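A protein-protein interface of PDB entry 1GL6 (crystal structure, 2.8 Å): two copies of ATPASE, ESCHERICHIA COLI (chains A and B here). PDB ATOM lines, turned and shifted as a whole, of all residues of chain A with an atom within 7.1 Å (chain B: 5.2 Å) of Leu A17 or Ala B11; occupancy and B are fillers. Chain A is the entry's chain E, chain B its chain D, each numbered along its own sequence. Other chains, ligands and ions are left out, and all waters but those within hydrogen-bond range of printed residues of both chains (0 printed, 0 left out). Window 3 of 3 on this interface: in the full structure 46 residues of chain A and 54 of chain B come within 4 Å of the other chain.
The backbone carbonyl oxygen of Leu A17 lies close to the backbone carbonyl oxygen of Gly B9 (3.1 Å).
Position printed for both chains: 13.
Of the 9 pairs that touch across the chains among the printed residues, none has its exchanged pair printed and touching as well.
Of chain B, only Gly B9 (3.1 Å) and Ala B11 (3.7 Å) come within 4 Å of Leu A17.
Of the printed residues of chain B, Arg A385 touches Arg B366 (3.9 Å).
Of the printed residues of chain A, Phe B8 touches Arg A18.
Of the printed residues of chain A, Ala B11 touches Leu A17 (3.7 Å) and Glu A363 (3.9 Å).
Pro B12 touches none of the printed residues of chain A.
Of the printed residues of chain A, Glu B388 touches Glu A363.
The nearest residue of chain B that does not touch Leu A17 is Gly B10 (4.3 Å).
Of the 13 printed residues of chain A, 4 touch a printed residue of chain B.
Hydrophobic or aromatic side chains of chain A that line the printed part of chain B: Leu A17.
Along chain A the printed residues that touch a printed residue of chain B span positions 17 to 385.
Of the 8 printed residues of chain B, 6 touch a printed residue of chain A.
Printed residues of chain B that touch a printed residue of chain A: Phe B8, Gly B9, Gly B10, Ala B11, Arg B366 and Glu B388.
Hydrophobic or aromatic side chains of chain B within 4 Å of the printed part of chain A: Phe B8 and Ala B11.
Ala B11 touches Leu A17 (CB to CD1, 3.7 Å).
Arg A18 touches Phe B8 (NH2 to CE1, 3.2 Å).
Arg A18 touches Gly B9 (CG to O, 3.1 Å).
Arg A18 touches Gly B10.
Gly B10 touches Glu A363.
OE1 of Glu A363 touches N of Ala B11, 3.9 Å away.
Glu B388 touches Glu A363 (OE1 to OE2, 3.9 Å).
Arg B366 touches Arg A385.
The guanidinium group of Arg B366 is in hydrogen-bond range of the backbone carbonyl oxygen of Ala B11 (2.8 Å).
The guanidinium group (NH2) of Arg B366 lies within salt-bridge range of the side-chain carboxylate (OE1) of Glu B388, at 2.8 Å.
N of Leu A17 is in hydrogen-bond range of O of Glu A363.
The side-chain carboxylate (OE1) of Glu A363 lies within salt-bridge range of the guanidinium group (NH1) of Arg A18, 3.1 Å away.
The guanidinium group (NH2) of Arg A385 is in salt-bridge range of the side-chain carboxylate (OE2) of Glu A365 (3.998 Å).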
ATOM      1  N   PHE A  13      11.519 -26.157 -11.698  1.00  0.00           N
ATOM      2  CA  PHE A  13      12.795 -26.775 -11.389  1.00  0.00           C
ATOM      3  C   PHE A  13      12.778 -28.285 -11.493  1.00  0.00           C
ATOM      4  O   PHE A  13      11.716 -28.923 -11.496  1.00  0.00           O
ATOM      5  CB  PHE A  13      13.260 -26.371  -9.999  1.00  0.00           C
ATOM      6  CG  PHE A  13      12.203 -26.492  -8.952  1.00  0.00           C
ATOM      7  CD1 PHE A  13      11.259 -25.491  -8.791  1.00  0.00           C
ATOM      8  CD2 PHE A  13      12.139 -27.614  -8.138  1.00  0.00           C
ATOM      9  CE1 PHE A  13      10.267 -25.603  -7.840  1.00  0.00           C
ATOM     10  CE2 PHE A  13      11.148 -27.738  -7.180  1.00  0.00           C
ATOM     11  CZ  PHE A  13      10.209 -26.730  -7.029  1.00  0.00           C
ATOM     12  N   ARG A  15      14.507 -30.444  -9.308  1.00  0.00           N
ATOM     13  CA  ARG A  15      14.438 -31.123  -8.019  1.00  0.00           C
ATOM     14  C   ARG A  15      14.471 -30.162  -6.842  1.00  0.00           C
ATOM     15  O   ARG A  15      15.246 -29.205  -6.834  1.00  0.00           O
ATOM     16  CB  ARG A  15      15.603 -32.109  -7.946  1.00  0.00           C
ATOM     17  CG  ARG A  15      15.957 -32.692  -6.588  1.00  0.00           C
ATOM     18  CD  ARG A  15      17.112 -33.675  -6.781  1.00  0.00           C
ATOM     19  NE  ARG A  15      17.806 -34.077  -5.558  1.00  0.00           N
ATOM     20  CZ  ARG A  15      17.228 -34.596  -4.478  1.00  0.00           C
ATOM     21  NH1 ARG A  15      15.913 -34.777  -4.427  1.00  0.00           N
ATOM     22  NH2 ARG A  15      17.983 -34.957  -3.446  1.00  0.00           N
ATOM     23  N   PHE A  16      13.621 -30.421  -5.853  1.00  0.00           N
ATOM     24  CA  PHE A  16      13.538 -29.594  -4.653  1.00  0.00           C
ATOM     25  C   PHE A  16      14.524 -30.106  -3.608  1.00  0.00           C
ATOM     26  O   PHE A  16      14.512 -31.280  -3.263  1.00  0.00           O
ATOM     27  CB  PHE A  16      12.105 -29.624  -4.111  1.00  0.00           C
ATOM     28  CG  PHE A  16      11.936 -28.963  -2.770  1.00  0.00           C
ATOM     29  CD1 PHE A  16      12.240 -29.651  -1.592  1.00  0.00           C
ATOM     30  CD2 PHE A  16      11.471 -27.653  -2.679  1.00  0.00           C
ATOM     31  CE1 PHE A  16      12.084 -29.051  -0.340  1.00  0.00           C
ATOM     32  CE2 PHE A  16      11.312 -27.043  -1.437  1.00  0.00           C
ATOM     33  CZ  PHE A  16      11.621 -27.748  -0.262  1.00  0.00           C
ATOM     34  N   LEU A  17      15.376 -29.215  -3.110  1.00  0.00           N
ATOM     35  CA  LEU A  17      16.376 -29.578  -2.121  1.00  0.00           C
ATOM     36  C   LEU A  17      15.975 -29.375  -0.650  1.00  0.00           C
ATOM     37  O   LEU A  17      15.895 -30.341   0.116  1.00  0.00           O
ATOM     38  CB  LEU A  17      17.694 -28.847  -2.409  1.00  0.00           C
ATOM     39  CG  LEU A  17      18.417 -29.283  -3.677  1.00  0.00           C
ATOM     40  CD1 LEU A  17      19.637 -28.395  -3.935  1.00  0.00           C
ATOM     41  CD2 LEU A  17      18.808 -30.732  -3.535  1.00  0.00           C
ATOM     42  N   ARG A  18      15.738 -28.131  -0.243  1.00  0.00           N
ATOM     43  CA  ARG A  18      15.359 -27.834   1.146  1.00  0.00           C
ATOM     44  C   ARG A  18      14.582 -26.525   1.224  1.00  0.00           C
ATOM     45  O   ARG A  18      14.455 -25.819   0.234  1.00  0.00           O
ATOM     46  CB  ARG A  18      16.616 -27.759   2.039  1.00  0.00           C
ATOM     47  CG  ARG A  18      17.895 -27.405   1.298  1.00  0.00           C
ATOM     48  CD  ARG A  18      18.567 -26.149   1.788  1.00  0.00           C
ATOM     49  NE  ARG A  18      19.448 -26.413   2.917  1.00  0.00           N
ATOM     50  CZ  ARG A  18      20.661 -25.884   3.074  1.00  0.00           C
ATOM     51  NH1 ARG A  18      21.172 -25.054   2.179  1.00  0.00           N
ATOM     52  NH2 ARG A  18      21.368 -26.175   4.146  1.00  0.00           N
ATOM     53  N   GLY A  19      14.042 -26.205   2.394  1.00  0.00           N
ATOM     54  CA  GLY A  19      13.320 -24.950   2.536  1.00  0.00           C
ATOM     55  C   GLY A  19      11.816 -25.029   2.385  1.00  0.00           C
ATOM     56  O   GLY A  19      11.220 -26.110   2.427  1.00  0.00           O
ATOM     57  N   HIS A 362      13.617 -21.329  -0.740  1.00  0.00           N
ATOM     58  CA  HIS A 362      13.792 -22.740  -0.966  1.00  0.00           C
ATOM     59  C   HIS A 362      15.092 -22.897  -1.731  1.00  0.00           C
ATOM     60  O   HIS A 362      15.554 -21.942  -2.362  1.00  0.00           O
ATOM     61  CB  HIS A 362      12.584 -23.343  -1.714  1.00  0.00           C
ATOM     62  CG  HIS A 362      12.371 -22.830  -3.106  1.00  0.00           C
ATOM     63  ND1 HIS A 362      11.242 -23.139  -3.838  1.00  0.00           N
ATOM     64  CD2 HIS A 362      13.149 -22.088  -3.928  1.00  0.00           C
ATOM     65  CE1 HIS A 362      11.336 -22.619  -5.044  1.00  0.00           C
ATOM     66  NE2 HIS A 362      12.490 -21.971  -5.128  1.00  0.00           N
ATOM     67  N   GLU A 363      15.742 -24.052  -1.608  1.00  0.00           N
ATOM     68  CA  GLU A 363      16.971 -24.303  -2.345  1.00  0.00           C
ATOM     69  C   GLU A 363      16.530 -25.353  -3.333  1.00  0.00           C
ATOM     70  O   GLU A 363      16.090 -26.445  -2.970  1.00  0.00           O
ATOM     71  CB  GLU A 363      18.100 -24.818  -1.444  1.00  0.00           C
ATOM     72  CG  GLU A 363      19.466 -24.645  -2.099  1.00  0.00           C
ATOM     73  CD  GLU A 363      20.633 -24.882  -1.159  1.00  0.00           C
ATOM     74  OE1 GLU A 363      20.836 -26.033  -0.729  1.00  0.00           O
ATOM     75  OE2 GLU A 363      21.358 -23.910  -0.854  1.00  0.00           O
ATOM     76  N   VAL A 364      16.639 -24.995  -4.598  1.00  0.00           N
ATOM     77  CA  VAL A 364      16.198 -25.838  -5.684  1.00  0.00           C
ATOM     78  C   VAL A 364      17.320 -26.174  -6.662  1.00  0.00           C
ATOM     79  O   VAL A 364      18.363 -25.524  -6.675  1.00  0.00           O
ATOM     80  CB  VAL A 364      15.021 -25.109  -6.368  1.00  0.00           C
ATOM     81  CG1 VAL A 364      15.152 -25.145  -7.841  1.00  0.00           C
ATOM     82  CG2 VAL A 364      13.722 -25.712  -5.908  1.00  0.00           C
ATOM     83  N   GLU A 365      17.101 -27.215  -7.459  1.00  0.00           N
ATOM     84  CA  GLU A 365      18.070 -27.664  -8.458  1.00  0.00           C
ATOM     85  C   GLU A 365      17.423 -27.534  -9.829  1.00  0.00           C
ATOM     86  O   GLU A 365      16.455 -28.214 -10.133  1.00  0.00           O
ATOM     87  CB  GLU A 365      18.430 -29.118  -8.195  1.00  0.00           C
ATOM     88  CG  GLU A 365      19.904 -29.395  -8.072  1.00  0.00           C
ATOM     89  CD  GLU A 365      20.172 -30.861  -7.776  1.00  0.00           C
ATOM     90  OE1 GLU A 365      19.583 -31.710  -8.480  1.00  0.00           O
ATOM     91  OE2 GLU A 365      20.968 -31.174  -6.854  1.00  0.00           O
ATOM     92  N   GLU A 384      22.154 -26.612 -11.634  1.00  0.00           N
ATOM     93  CA  GLU A 384      22.544 -25.426 -10.851  1.00  0.00           C
ATOM     94  C   GLU A 384      21.716 -25.266  -9.557  1.00  0.00           C
ATOM     95  O   GLU A 384      20.491 -25.230  -9.626  1.00  0.00           O
ATOM     96  CB  GLU A 384      22.375 -24.158 -11.696  1.00  0.00           C
ATOM     97  CG  GLU A 384      20.921 -23.775 -11.966  1.00  0.00           C
ATOM     98  CD  GLU A 384      20.787 -22.439 -12.690  1.00  0.00           C
ATOM     99  OE1 GLU A 384      19.645 -21.937 -12.837  1.00  0.00           O
ATOM    100  OE2 GLU A 384      21.823 -21.891 -13.116  1.00  0.00           O
ATOM    101  N   ARG A 385      22.358 -25.171  -8.386  1.00  0.00           N
ATOM    102  CA  ARG A 385      21.596 -24.994  -7.141  1.00  0.00           C
ATOM    103  C   ARG A 385      21.266 -23.512  -6.970  1.00  0.00           C
ATOM    104  O   ARG A 385      22.138 -22.648  -7.070  1.00  0.00           O
ATOM    105  CB  ARG A 385      22.354 -25.495  -5.896  1.00  0.00           C
ATOM    106  CG  ARG A 385      23.721 -26.080  -6.144  1.00  0.00           C
ATOM    107  CD  ARG A 385      23.682 -27.411  -6.894  1.00  0.00           C
ATOM    108  NE  ARG A 385      24.979 -27.710  -7.505  1.00  0.00           N
ATOM    109  CZ  ARG A 385      25.406 -28.903  -7.918  1.00  0.00           C
ATOM    110  NH1 ARG A 385      26.610 -28.996  -8.456  1.00  0.00           N
ATOM    111  NH2 ARG A 385      24.674 -29.999  -7.786  1.00  0.00           N
ATOM    112  N   VAL A 386      19.994 -23.231  -6.706  1.00  0.00           N
ATOM    113  CA  VAL A 386      19.517 -21.870  -6.548  1.00  0.00           C
ATOM    114  C   VAL A 386      18.693 -21.698  -5.288  1.00  0.00           C
ATOM    115  O   VAL A 386      17.815 -22.501  -5.013  1.00  0.00           O
ATOM    116  CB  VAL A 386      18.661 -21.489  -7.744  1.00  0.00           C
ATOM    117  CG1 VAL A 386      17.988 -20.157  -7.509  1.00  0.00           C
ATOM    118  CG2 VAL A 386      19.525 -21.441  -8.979  1.00  0.00           C
ATOM    119  N   PHE B   8      22.472 -33.668   5.654  1.00  0.00           N
ATOM    120  CA  PHE B   8      22.482 -32.288   5.179  1.00  0.00           C
ATOM    121  C   PHE B   8      21.337 -32.100   4.184  1.00  0.00           C
ATOM    122  O   PHE B   8      21.268 -32.797   3.173  1.00  0.00           O
ATOM    123  CB  PHE B   8      23.831 -31.996   4.504  1.00  0.00           C
ATOM    124  CG  PHE B   8      23.905 -30.655   3.830  1.00  0.00           C
ATOM    125  CD1 PHE B   8      23.751 -29.482   4.552  1.00  0.00           C
ATOM    126  CD2 PHE B   8      24.125 -30.565   2.462  1.00  0.00           C
ATOM    127  CE1 PHE B   8      23.817 -28.237   3.916  1.00  0.00           C
ATOM    128  CE2 PHE B   8      24.195 -29.320   1.817  1.00  0.00           C
ATOM    129  CZ  PHE B   8      24.037 -28.161   2.546  1.00  0.00           C
ATOM    130  N   GLY B   9      20.448 -31.156   4.474  1.00  0.00           N
ATOM    131  CA  GLY B   9      19.303 -30.903   3.613  1.00  0.00           C
ATOM    132  C   GLY B   9      19.566 -30.293   2.242  1.00  0.00           C
ATOM    133  O   GLY B   9      18.699 -30.357   1.365  1.00  0.00           O
ATOM    134  N   GLY B  10      20.737 -29.695   2.040  1.00  0.00           N
ATOM    135  CA  GLY B  10      21.042 -29.094   0.755  1.00  0.00           C
ATOM    136  C   GLY B  10      21.534 -30.102  -0.260  1.00  0.00           C
ATOM    137  O   GLY B  10      21.353 -31.312  -0.082  1.00  0.00           O
ATOM    138  N   ALA B  11      22.157 -29.604  -1.329  1.00  0.00           N
ATOM    139  CA  ALA B  11      22.689 -30.461  -2.391  1.00  0.00           C
ATOM    140  C   ALA B  11      23.897 -31.251  -1.885  1.00  0.00           C
ATOM    141  O   ALA B  11      24.813 -30.671  -1.290  1.00  0.00           O
ATOM    142  CB  ALA B  11      23.084 -29.606  -3.591  1.00  0.00           C
ATOM    143  N   PRO B  12      23.917 -32.586  -2.113  1.00  0.00           N
ATOM    144  CA  PRO B  12      25.050 -33.402  -1.651  1.00  0.00           C
ATOM    145  C   PRO B  12      26.333 -32.850  -2.228  1.00  0.00           C
ATOM    146  O   PRO B  12      26.331 -32.225  -3.289  1.00  0.00           O
ATOM    147  CB  PRO B  12      24.738 -34.793  -2.196  1.00  0.00           C
ATOM    148  CG  PRO B  12      23.251 -34.786  -2.323  1.00  0.00           C
ATOM    149  CD  PRO B  12      22.960 -33.412  -2.868  1.00  0.00           C
ATOM    150  N   PHE B  13      27.438 -33.088  -1.541  1.00  0.00           N
ATOM    151  CA  PHE B  13      28.700 -32.576  -2.026  1.00  0.00           C
ATOM    152  C   PHE B  13      29.788 -33.617  -2.096  1.00  0.00           C
ATOM    153  O   PHE B  13      29.701 -34.689  -1.486  1.00  0.00           O
ATOM    154  CB  PHE B  13      29.163 -31.402  -1.160  1.00  0.00           C
ATOM    155  CG  PHE B  13      29.105 -31.674   0.310  1.00  0.00           C
ATOM    156  CD1 PHE B  13      27.913 -31.521   1.007  1.00  0.00           C
ATOM    157  CD2 PHE B  13      30.234 -32.099   0.995  1.00  0.00           C
ATOM    158  CE1 PHE B  13      27.847 -31.787   2.368  1.00  0.00           C
ATOM    159  CE2 PHE B  13      30.181 -32.368   2.353  1.00  0.00           C
ATOM    160  CZ  PHE B  13      28.983 -32.212   3.042  1.00  0.00           C
ATOM    161  N   ARG B 366      31.545 -29.058  -4.455  1.00  0.00           N
ATOM    162  CA  ARG B 366      30.563 -29.860  -5.177  1.00  0.00           C
ATOM    163  C   ARG B 366      30.851 -30.047  -6.660  1.00  0.00           C
ATOM    164  O   ARG B 366      31.541 -29.231  -7.274  1.00  0.00           O
ATOM    165  CB  ARG B 366      29.174 -29.236  -5.037  1.00  0.00           C
ATOM    166  CG  ARG B 366      28.232 -29.939  -4.057  1.00  0.00           C
ATOM    167  CD  ARG B 366      26.781 -29.501  -4.287  1.00  0.00           C
ATOM    168  NE  ARG B 366      26.567 -28.087  -3.999  1.00  0.00           N
ATOM    169  CZ  ARG B 366      26.356 -27.591  -2.783  1.00  0.00           C
ATOM    170  NH1 ARG B 366      26.321 -28.394  -1.721  1.00  0.00           N
ATOM    171  NH2 ARG B 366      26.177 -26.283  -2.631  1.00  0.00           N
ATOM    172  N   GLU B 388      27.743 -22.130   2.513  1.00  0.00           N
ATOM    173  CA  GLU B 388      26.301 -22.131   2.710  1.00  0.00           C
ATOM    174  C   GLU B 388      25.845 -22.525   4.110  1.00  0.00           C
ATOM    175  O   GLU B 388      26.568 -23.197   4.848  1.00  0.00           O
ATOM    176  CB  GLU B 388      25.660 -23.068   1.687  1.00  0.00           C
ATOM    177  CG  GLU B 388      26.414 -24.365   1.495  1.00  0.00           C
ATOM    178  CD  GLU B 388      25.730 -25.284   0.525  1.00  0.00           C
ATOM    179  OE1 GLU B 388      25.163 -24.779  -0.461  1.00  0.00           O
ATOM    180  OE2 GLU B 388      25.772 -26.513   0.741  1.00  0.00           O
